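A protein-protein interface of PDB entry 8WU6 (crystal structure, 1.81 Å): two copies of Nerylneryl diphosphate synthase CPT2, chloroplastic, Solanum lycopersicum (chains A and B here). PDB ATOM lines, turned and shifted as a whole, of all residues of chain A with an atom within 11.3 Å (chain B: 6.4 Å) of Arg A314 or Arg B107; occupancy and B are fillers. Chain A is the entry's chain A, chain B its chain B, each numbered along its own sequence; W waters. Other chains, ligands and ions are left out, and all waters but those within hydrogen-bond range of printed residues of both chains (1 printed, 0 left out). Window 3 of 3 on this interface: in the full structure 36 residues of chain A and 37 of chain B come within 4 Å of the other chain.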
ATOM      1  N   LEU A  93       5.784   6.905 -16.206  1.00  0.00           N
ATOM      2  CA  LEU A  93       5.474   6.593 -14.813  1.00  0.00           C
ATOM      3  C   LEU A  93       4.118   5.914 -14.615  1.00  0.00           C
ATOM      4  O   LEU A  93       3.276   6.444 -13.893  1.00  0.00           O
ATOM      5  CB  LEU A  93       5.528   7.848 -13.945  1.00  0.00           C
ATOM      6  CG  LEU A  93       6.825   8.653 -13.897  1.00  0.00           C
ATOM      7  CD1 LEU A  93       6.688   9.866 -12.965  1.00  0.00           C
ATOM      8  CD2 LEU A  93       7.958   7.746 -13.461  1.00  0.00           C
ATOM      9  N   GLU A 285       3.496   1.933  -3.000  1.00  0.00           N
ATOM     10  CA  GLU A 285       2.787   3.164  -2.637  1.00  0.00           C
ATOM     11  C   GLU A 285       1.362   2.857  -2.171  1.00  0.00           C
ATOM     12  O   GLU A 285       0.606   2.178  -2.876  1.00  0.00           O
ATOM     13  CB  GLU A 285       2.744   4.087  -3.855  1.00  0.00           C
ATOM     14  CG  GLU A 285       4.038   4.773  -4.100  1.00  0.00           C
ATOM     15  CD  GLU A 285       4.220   6.033  -3.247  1.00  0.00           C
ATOM     16  OE1 GLU A 285       3.346   6.403  -2.413  1.00  0.00           O
ATOM     17  OE2 GLU A 285       5.281   6.643  -3.421  1.00  0.00           O
ATOM     18  N   ILE A 305      -3.569   7.068 -10.258  1.00  0.00           N
ATOM     19  CA  ILE A 305      -2.332   7.053 -11.043  1.00  0.00           C
ATOM     20  C   ILE A 305      -1.678   8.433 -11.048  1.00  0.00           C
ATOM     21  O   ILE A 305      -0.456   8.554 -10.896  1.00  0.00           O
ATOM     22  CB  ILE A 305      -2.622   6.562 -12.467  1.00  0.00           C
ATOM     23  CG1 ILE A 305      -3.063   5.099 -12.427  1.00  0.00           C
ATOM     24  CG2 ILE A 305      -1.399   6.737 -13.378  1.00  0.00           C
ATOM     25  CD1 ILE A 305      -3.595   4.618 -13.751  1.00  0.00           C
ATOM     26  N   LEU A 306      -2.475   9.500 -11.182  1.00  0.00           N
ATOM     27  CA  LEU A 306      -1.894  10.841 -11.115  1.00  0.00           C
ATOM     28  C   LEU A 306      -1.227  11.074  -9.766  1.00  0.00           C
ATOM     29  O   LEU A 306      -0.119  11.621  -9.690  1.00  0.00           O
ATOM     30  CB  LEU A 306      -2.972  11.906 -11.361  1.00  0.00           C
ATOM     31  CG  LEU A 306      -2.517  13.368 -11.183  1.00  0.00           C
ATOM     32  CD1 LEU A 306      -1.368  13.711 -12.128  1.00  0.00           C
ATOM     33  CD2 LEU A 306      -3.660  14.373 -11.299  1.00  0.00           C
ATOM     34  N   ASN A 307      -1.874  10.643  -8.686  1.00  0.00           N
ATOM     35  CA  ASN A 307      -1.278  10.818  -7.365  1.00  0.00           C
ATOM     36  C   ASN A 307       0.015  10.012  -7.241  1.00  0.00           C
ATOM     37  O   ASN A 307       1.016  10.500  -6.699  1.00  0.00           O
ATOM     38  CB  ASN A 307      -2.289  10.412  -6.294  1.00  0.00           C
ATOM     39  CG  ASN A 307      -1.729  10.510  -4.897  1.00  0.00           C
ATOM     40  OD1 ASN A 307      -1.542   9.507  -4.207  1.00  0.00           O
ATOM     41  ND2 ASN A 307      -1.478  11.743  -4.458  1.00  0.00           N
ATOM     42  N   PHE A 308       0.011   8.775  -7.754  1.00  0.00           N
ATOM     43  CA  PHE A 308       1.222   7.959  -7.812  1.00  0.00           C
ATOM     44  C   PHE A 308       2.354   8.679  -8.550  1.00  0.00           C
ATOM     45  O   PHE A 308       3.508   8.682  -8.091  1.00  0.00           O
ATOM     46  CB  PHE A 308       0.866   6.623  -8.496  1.00  0.00           C
ATOM     47  CG  PHE A 308       2.053   5.760  -8.836  1.00  0.00           C
ATOM     48  CD1 PHE A 308       2.605   4.915  -7.881  1.00  0.00           C
ATOM     49  CD2 PHE A 308       2.598   5.781 -10.111  1.00  0.00           C
ATOM     50  CE1 PHE A 308       3.705   4.099  -8.194  1.00  0.00           C
ATOM     51  CE2 PHE A 308       3.690   4.984 -10.424  1.00  0.00           C
ATOM     52  CZ  PHE A 308       4.233   4.139  -9.460  1.00  0.00           C
ATOM     53  N   GLN A 309       2.040   9.327  -9.676  1.00  0.00           N
ATOM     54  CA  GLN A 309       3.070  10.024 -10.454  1.00  0.00           C
ATOM     55  C   GLN A 309       3.619  11.238  -9.706  1.00  0.00           C
ATOM     56  O   GLN A 309       4.832  11.490  -9.715  1.00  0.00           O
ATOM     57  CB  GLN A 309       2.485  10.451 -11.792  1.00  0.00           C
ATOM     58  CG  GLN A 309       2.134   9.275 -12.675  1.00  0.00           C
ATOM     59  CD  GLN A 309       1.316   9.697 -13.894  1.00  0.00           C
ATOM     60  OE1 GLN A 309       0.702  10.779 -13.915  1.00  0.00           O
ATOM     61  NE2 GLN A 309       1.299   8.844 -14.909  1.00  0.00           N
ATOM     62  N   GLN A 310       2.741  11.998  -9.052  1.00  0.00           N
ATOM     63  CA  GLN A 310       3.185  13.159  -8.283  1.00  0.00           C
ATOM     64  C   GLN A 310       4.072  12.730  -7.124  1.00  0.00           C
ATOM     65  O   GLN A 310       5.120  13.338  -6.867  1.00  0.00           O
ATOM     66  CB  GLN A 310       1.961  13.896  -7.750  1.00  0.00           C
ATOM     67  CG  GLN A 310       1.094  14.568  -8.846  1.00  0.00           C
ATOM     68  CD  GLN A 310      -0.204  15.111  -8.264  1.00  0.00           C
ATOM     69  OE1 GLN A 310      -0.612  14.723  -7.165  1.00  0.00           O
ATOM     70  NE2 GLN A 310      -0.848  16.010  -8.982  1.00  0.00           N
ATOM     71  N   ARG A 311       3.680  11.663  -6.427  1.00  0.00           N
ATOM     72  CA  ARG A 311       4.503  11.169  -5.326  1.00  0.00           C
ATOM     73  C   ARG A 311       5.864  10.698  -5.813  1.00  0.00           C
ATOM     74  O   ARG A 311       6.871  10.885  -5.122  1.00  0.00           O
ATOM     75  CB  ARG A 311       3.802  10.026  -4.597  1.00  0.00           C
ATOM     76  CG  ARG A 311       2.493  10.369  -3.905  1.00  0.00           C
ATOM     77  CD  ARG A 311       1.963   9.001  -3.491  1.00  0.00           C
ATOM     78  NE  ARG A 311       0.628   8.944  -2.906  1.00  0.00           N
ATOM     79  CZ  ARG A 311       0.214   7.930  -2.154  1.00  0.00           C
ATOM     80  NH1 ARG A 311       1.017   6.923  -1.853  1.00  0.00           N
ATOM     81  NH2 ARG A 311      -1.039   7.909  -1.723  1.00  0.00           N
ATOM     82  N   HIS A 312       5.913  10.067  -6.989  1.00  0.00           N
ATOM     83  CA  HIS A 312       7.192   9.602  -7.522  1.00  0.00           C
ATOM     84  C   HIS A 312       8.143  10.760  -7.813  1.00  0.00           C
ATOM     85  O   HIS A 312       9.346  10.658  -7.551  1.00  0.00           O
ATOM     86  CB  HIS A 312       6.990   8.797  -8.800  1.00  0.00           C
ATOM     87  CG  HIS A 312       8.282   8.332  -9.391  1.00  0.00           C
ATOM     88  ND1 HIS A 312       8.845   8.914 -10.506  1.00  0.00           N
ATOM     89  CD2 HIS A 312       9.131   7.350  -9.007  1.00  0.00           C
ATOM     90  CE1 HIS A 312       9.988   8.312 -10.782  1.00  0.00           C
ATOM     91  NE2 HIS A 312      10.181   7.356  -9.892  1.00  0.00           N
ATOM     92  N   ARG A 313       7.630  11.855  -8.380  1.00  0.00           N
ATOM     93  CA  ARG A 313       8.471  13.030  -8.617  1.00  0.00           C
ATOM     94  C   ARG A 313       8.907  13.677  -7.311  1.00  0.00           C
ATOM     95  O   ARG A 313      10.002  14.257  -7.232  1.00  0.00           O
ATOM     96  CB  ARG A 313       7.743  14.039  -9.490  1.00  0.00           C
ATOM     97  CG  ARG A 313       7.406  13.503 -10.882  1.00  0.00           C
ATOM     98  CD  ARG A 313       6.982  14.631 -11.803  1.00  0.00           C
ATOM     99  NE  ARG A 313       5.593  15.032 -11.578  1.00  0.00           N
ATOM    100  CZ  ARG A 313       4.550  14.502 -12.199  1.00  0.00           C
ATOM    101  NH1 ARG A 313       4.696  13.553 -13.113  1.00  0.00           N
ATOM    102  NH2 ARG A 313       3.329  14.931 -11.892  1.00  0.00           N
ATOM    103  N   ARG A 314       8.063  13.595  -6.282  1.00  0.00           N
ATOM    104  CA  ARG A 314       8.375  14.270  -5.029  1.00  0.00           C
ATOM    105  C   ARG A 314       9.475  13.538  -4.280  1.00  0.00           C
ATOM    106  O   ARG A 314      10.417  14.167  -3.778  1.00  0.00           O
ATOM    107  CB  ARG A 314       7.113  14.383  -4.168  1.00  0.00           C
ATOM    108  CG  ARG A 314       7.408  14.839  -2.735  1.00  0.00           C
ATOM    109  CD  ARG A 314       6.171  15.280  -1.992  1.00  0.00           C
ATOM    110  NE  ARG A 314       6.534  15.814  -0.683  1.00  0.00           N
ATOM    111  CZ  ARG A 314       5.740  15.843   0.375  1.00  0.00           C
ATOM    112  NH1 ARG A 314       4.492  15.410   0.317  1.00  0.00           N
ATOM    113  NH2 ARG A 314       6.191  16.378   1.504  1.00  0.00           N
ATOM    114  N   PHE A 315       9.397  12.210  -4.224  1.00  0.00           N
ATOM    115  CA  PHE A 315      10.337  11.399  -3.451  1.00  0.00           C
ATOM    116  C   PHE A 315      11.173  10.492  -4.354  1.00  0.00           C
ATOM    117  O   PHE A 315      12.209   9.975  -3.922  1.00  0.00           O
ATOM    118  CB  PHE A 315       9.588  10.550  -2.418  1.00  0.00           C
ATOM    119  CG  PHE A 315       8.771  11.346  -1.445  1.00  0.00           C
ATOM    120  CD1 PHE A 315       9.382  12.073  -0.438  1.00  0.00           C
ATOM    121  CD2 PHE A 315       7.384  11.349  -1.523  1.00  0.00           C
ATOM    122  CE1 PHE A 315       8.637  12.807   0.453  1.00  0.00           C
ATOM    123  CE2 PHE A 315       6.633  12.059  -0.615  1.00  0.00           C
ATOM    124  CZ  PHE A 315       7.261  12.801   0.366  1.00  0.00           C
ATOM    125  N   ASP B 103      11.284   9.741   9.424  1.00  0.00           N
ATOM    126  CA  ASP B 103      11.778  10.315   8.179  1.00  0.00           C
ATOM    127  C   ASP B 103      11.713  11.834   8.223  1.00  0.00           C
ATOM    128  O   ASP B 103      10.879  12.421   8.919  1.00  0.00           O
ATOM    129  CB  ASP B 103      10.951   9.782   7.006  1.00  0.00           C
ATOM    130  CG  ASP B 103      11.740   9.685   5.697  1.00  0.00           C
ATOM    131  OD1 ASP B 103      12.964   9.948   5.702  1.00  0.00           O
ATOM    132  OD2 ASP B 103      11.108   9.431   4.631  1.00  0.00           O
ATOM    133  N   GLY B 104      12.605  12.467   7.464  1.00  0.00           N
ATOM    134  CA  GLY B 104      12.620  13.912   7.334  1.00  0.00           C
ATOM    135  C   GLY B 104      13.801  14.610   7.983  1.00  0.00           C
ATOM    136  O   GLY B 104      13.869  15.842   7.907  1.00  0.00           O
ATOM    137  N   ASN B 105      14.739  13.875   8.609  1.00  0.00           N
ATOM    138  CA  ASN B 105      15.850  14.531   9.306  1.00  0.00           C
ATOM    139  C   ASN B 105      16.750  15.301   8.347  1.00  0.00           C
ATOM    140  O   ASN B 105      17.202  16.406   8.666  1.00  0.00           O
ATOM    141  CB  ASN B 105      16.703  13.510  10.074  1.00  0.00           C
ATOM    142  CG  ASN B 105      15.983  12.908  11.259  1.00  0.00           C
ATOM    143  OD1 ASN B 105      15.058  13.493  11.794  1.00  0.00           O
ATOM    144  ND2 ASN B 105      16.419  11.729  11.680  1.00  0.00           N
ATOM    145  N   ARG B 106      17.058  14.716   7.189  1.00  0.00           N
ATOM    146  CA  ARG B 106      17.951  15.369   6.230  1.00  0.00           C
ATOM    147  C   ARG B 106      17.307  16.616   5.628  1.00  0.00           C
ATOM    148  O   ARG B 106      17.928  17.685   5.565  1.00  0.00           O
ATOM    149  CB  ARG B 106      18.327  14.381   5.124  1.00  0.00           C
ATOM    150  CG  ARG B 106      19.554  13.530   5.425  1.00  0.00           C
ATOM    151  CD  ARG B 106      19.749  12.452   4.353  1.00  0.00           C
ATOM    152  NE  ARG B 106      19.839  11.122   4.941  1.00  0.00           N
ATOM    153  CZ  ARG B 106      18.920  10.177   4.788  1.00  0.00           C
ATOM    154  NH1 ARG B 106      17.869  10.353   3.998  1.00  0.00           N
ATOM    155  NH2 ARG B 106      19.074   9.013   5.422  1.00  0.00           N
ATOM    156  N   ARG B 107      16.067  16.492   5.153  1.00  0.00           N
ATOM    157  CA  ARG B 107      15.365  17.643   4.585  1.00  0.00           C
ATOM    158  C   ARG B 107      15.185  18.747   5.617  1.00  0.00           C
ATOM    159  O   ARG B 107      15.285  19.938   5.293  1.00  0.00           O
ATOM    160  CB  ARG B 107      14.022  17.186   4.008  1.00  0.00           C
ATOM    161  CG  ARG B 107      14.207  16.120   2.933  1.00  0.00           C
ATOM    162  CD  ARG B 107      13.143  15.022   2.982  1.00  0.00           C
ATOM    163  NE  ARG B 107      11.781  15.521   2.895  1.00  0.00           N
ATOM    164  CZ  ARG B 107      10.704  14.783   3.128  1.00  0.00           C
ATOM    165  NH1 ARG B 107      10.800  13.513   3.499  1.00  0.00           N
ATOM    166  NH2 ARG B 107       9.500  15.334   2.977  1.00  0.00           N
ATOM    167  N   TRP B 108      14.931  18.375   6.871  1.00  0.00           N
ATOM    168  CA  TRP B 108      14.791  19.377   7.922  1.00  0.00           C
ATOM    169  C   TRP B 108      16.080  20.176   8.089  1.00  0.00           C
ATOM    170  O   TRP B 108      16.054  21.411   8.158  1.00  0.00           O
ATOM    171  CB  TRP B 108      14.396  18.692   9.234  1.00  0.00           C
ATOM    172  CG  TRP B 108      14.206  19.611  10.392  1.00  0.00           C
ATOM    173  CD1 TRP B 108      13.039  20.176  10.806  1.00  0.00           C
ATOM    174  CD2 TRP B 108      15.214  20.036  11.327  1.00  0.00           C
ATOM    175  NE1 TRP B 108      13.257  20.943  11.931  1.00  0.00           N
ATOM    176  CE2 TRP B 108      14.583  20.873  12.268  1.00  0.00           C
ATOM    177  CE3 TRP B 108      16.584  19.801  11.444  1.00  0.00           C
ATOM    178  CZ2 TRP B 108      15.277  21.475  13.323  1.00  0.00           C
ATOM    179  CZ3 TRP B 108      17.272  20.394  12.503  1.00  0.00           C
ATOM    180  CH2 TRP B 108      16.616  21.231  13.415  1.00  0.00           C
ATOM    181  N   ALA B 109      17.224  19.487   8.130  1.00  0.00           N
ATOM    182  CA  ALA B 109      18.487  20.193   8.334  1.00  0.00           C
ATOM    183  C   ALA B 109      18.791  21.103   7.154  1.00  0.00           C
ATOM    184  O   ALA B 109      19.246  22.239   7.334  1.00  0.00           O
ATOM    185  CB  ALA B 109      19.625  19.197   8.553  1.00  0.00           C
ATOM    186  N   LYS B 110      18.542  20.616   5.937  1.00  0.00           N
ATOM    187  CA  LYS B 110      18.741  21.437   4.748  1.00  0.00           C
ATOM    188  C   LYS B 110      17.885  22.696   4.786  1.00  0.00           C
ATOM    189  O   LYS B 110      18.366  23.795   4.475  1.00  0.00           O
ATOM    190  CB  LYS B 110      18.408  20.616   3.507  1.00  0.00           C
ATOM    191  CG  LYS B 110      19.603  20.185   2.703  1.00  0.00           C
ATOM    192  CD  LYS B 110      19.952  21.234   1.653  1.00  0.00           C
ATOM    193  CE  LYS B 110      18.900  21.249   0.547  1.00  0.00           C
ATOM    194  NZ  LYS B 110      19.337  22.024  -0.648  1.00  0.00           N
ATOM    195  N   ALA B 111      16.614  22.557   5.177  1.00  0.00           N
ATOM    196  CA  ALA B 111      15.714  23.704   5.243  1.00  0.00           C
ATOM    197  C   ALA B 111      16.144  24.694   6.312  1.00  0.00           C
ATOM    198  O   ALA B 111      15.893  25.899   6.179  1.00  0.00           O
ATOM    199  CB  ALA B 111      14.284  23.234   5.506  1.00  0.00           C
ATOM    200  N   LYS B 112      16.825  24.213   7.347  1.00  0.00           N
ATOM    201  CA  LYS B 112      17.242  25.012   8.488  1.00  0.00           C
ATOM    202  C   LYS B 112      18.599  25.669   8.283  1.00  0.00           C
ATOM    203  O   LYS B 112      19.018  26.467   9.130  1.00  0.00           O
ATOM    204  CB  LYS B 112      17.313  24.124   9.741  1.00  0.00           C
ATOM    205  CG  LYS B 112      16.240  24.349  10.796  1.00  0.00           C
ATOM    206  CD  LYS B 112      14.838  24.338  10.217  1.00  0.00           C
ATOM    207  CE  LYS B 112      13.816  24.735  11.276  1.00  0.00           C
ATOM    208  NZ  LYS B 112      12.478  25.041  10.690  1.00  0.00           N
ATOM    209  N   THR B 267       6.646  10.049   9.530  1.00  0.00           N
ATOM    210  CA  THR B 267       6.815  11.473   9.269  1.00  0.00           C
ATOM    211  C   THR B 267       7.487  11.687   7.908  1.00  0.00           C
ATOM    212  O   THR B 267       8.080  10.773   7.325  1.00  0.00           O
ATOM    213  CB  THR B 267       7.661  12.104  10.385  1.00  0.00           C
ATOM    214  OG1 THR B 267       8.891  11.370  10.521  1.00  0.00           O
ATOM    215  CG2 THR B 267       6.909  12.068  11.708  1.00  0.00           C
ATOM    216  N   GLY B 268       7.385  12.910   7.399  1.00  0.00           N
ATOM    217  CA  GLY B 268       8.104  13.286   6.195  1.00  0.00           C
ATOM    218  C   GLY B 268       7.326  13.169   4.898  1.00  0.00           C
ATOM    219  O   GLY B 268       7.856  13.553   3.844  1.00  0.00           O
ATOM    220  N   GLY B 269       6.113  12.629   4.934  1.00  0.00           N
ATOM    221  CA  GLY B 269       5.187  12.685   3.820  1.00  0.00           C
ATOM    222  C   GLY B 269       5.121  11.464   2.923  1.00  0.00           C
ATOM    223  O   GLY B 269       4.151  11.335   2.171  1.00  0.00           O
ATOM    224  N   GLU B 270       6.084  10.553   2.980  1.00  0.00           N
ATOM    225  CA  GLU B 270       6.021   9.396   2.086  1.00  0.00           C
ATOM    226  C   GLU B 270       4.988   8.402   2.602  1.00  0.00           C
ATOM    227  O   GLU B 270       4.870   8.205   3.816  1.00  0.00           O
ATOM    228  CB  GLU B 270       7.390   8.716   1.972  1.00  0.00           C
ATOM    229  CG  GLU B 270       7.653   8.148   0.589  1.00  0.00           C
ATOM    230  CD  GLU B 270       9.142   7.968   0.297  1.00  0.00           C
ATOM    231  OE1 GLU B 270       9.976   8.708   0.874  1.00  0.00           O
ATOM    232  OE2 GLU B 270       9.473   7.156  -0.581  1.00  0.00           O
ATOM    233  N   ASN B 290       3.022  14.960   6.736  1.00  0.00           N
ATOM    234  CA  ASN B 290       4.100  15.728   6.112  1.00  0.00           C
ATOM    235  C   ASN B 290       5.058  16.355   7.115  1.00  0.00           C
ATOM    236  O   ASN B 290       6.160  16.762   6.722  1.00  0.00           O
ATOM    237  CB  ASN B 290       3.519  16.824   5.225  1.00  0.00           C
ATOM    238  CG  ASN B 290       3.073  16.295   3.897  1.00  0.00           C
ATOM    239  OD1 ASN B 290       3.836  15.625   3.223  1.00  0.00           O
ATOM    240  ND2 ASN B 290       1.850  16.622   3.489  1.00  0.00           N
ATOM    241  N   LEU B 292       7.997  16.972   9.427  1.00  0.00           N
ATOM    242  CA  LEU B 292       9.316  16.336   9.464  1.00  0.00           C
ATOM    243  C   LEU B 292       9.629  15.880  10.884  1.00  0.00           C
ATOM    244  O   LEU B 292       9.197  16.498  11.853  1.00  0.00           O
ATOM    245  CB  LEU B 292      10.400  17.287   8.951  1.00  0.00           C
ATOM    246  CG  LEU B 292      10.153  17.897   7.556  1.00  0.00           C
ATOM    247  CD1 LEU B 292      11.251  18.883   7.243  1.00  0.00           C
ATOM    248  CD2 LEU B 292      10.157  16.810   6.488  1.00  0.00           C
HETATM  249  O   HOH W   1       7.528  17.185   4.150  1.00  0.00           O
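The side-chain amide oxygen (OD1) of Asn B290 is in hydrogen-bond range of the guanidinium group (NH1) of Arg A314 (3.0 Å).
The backbone carbonyl oxygen of Gly B268 sits at hydrogen-bond distance from the guanidinium group of Arg B107 (2.6 Å).
Among the printed residues, pairs that only touch across the chains: Phe A315 with Gly B268 (3.6 Å), Phe A315 with Gly B269 (3.6 Å), Phe A315 with Glu B270 (3.6 Å), Phe A315 with Arg B107 (3.7 Å) and Arg A314 with Arg B107 (3.8 Å).
Arg B107 touches two residues of chain A. Asp B103 touches none of the printed residues of chain A. No residue of chain A comes within 4 Å of Gly B104. No residue of chain A comes within 4 Å of Ala B109. No residue of chain A comes within 4 Å of Ala B111. Of chain A, only Phe A315 (3.6 Å) comes within 4 Å of Gly B268. Of chain A, only Arg A314 (3.0 Å) comes within 4 Å of Asn B290. Printed residues of chain A within 4 Å of Glu B270: Phe A315. Of the printed residues of chain B, Phe A315 touches Arg B107, Gly B268, Gly B269 and Glu B270. The nearest residue of chain A that does not touch Arg B107 is Arg A311 (9.6 Å).
Printed residues of chain A that touch a printed residue of chain B: Arg A314 and Phe A315. Hydrophobic or aromatic side chains of chain A within 4 Å of the printed part of chain B: Phe A315.
No position is printed for both chains.
Water W1 lies within hydrogen-bond range of O of Asn B290 (2.9 Å), NH2 of Arg B107 (2.9 Å) and NH2 of Arg A314 (3.1 Å).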
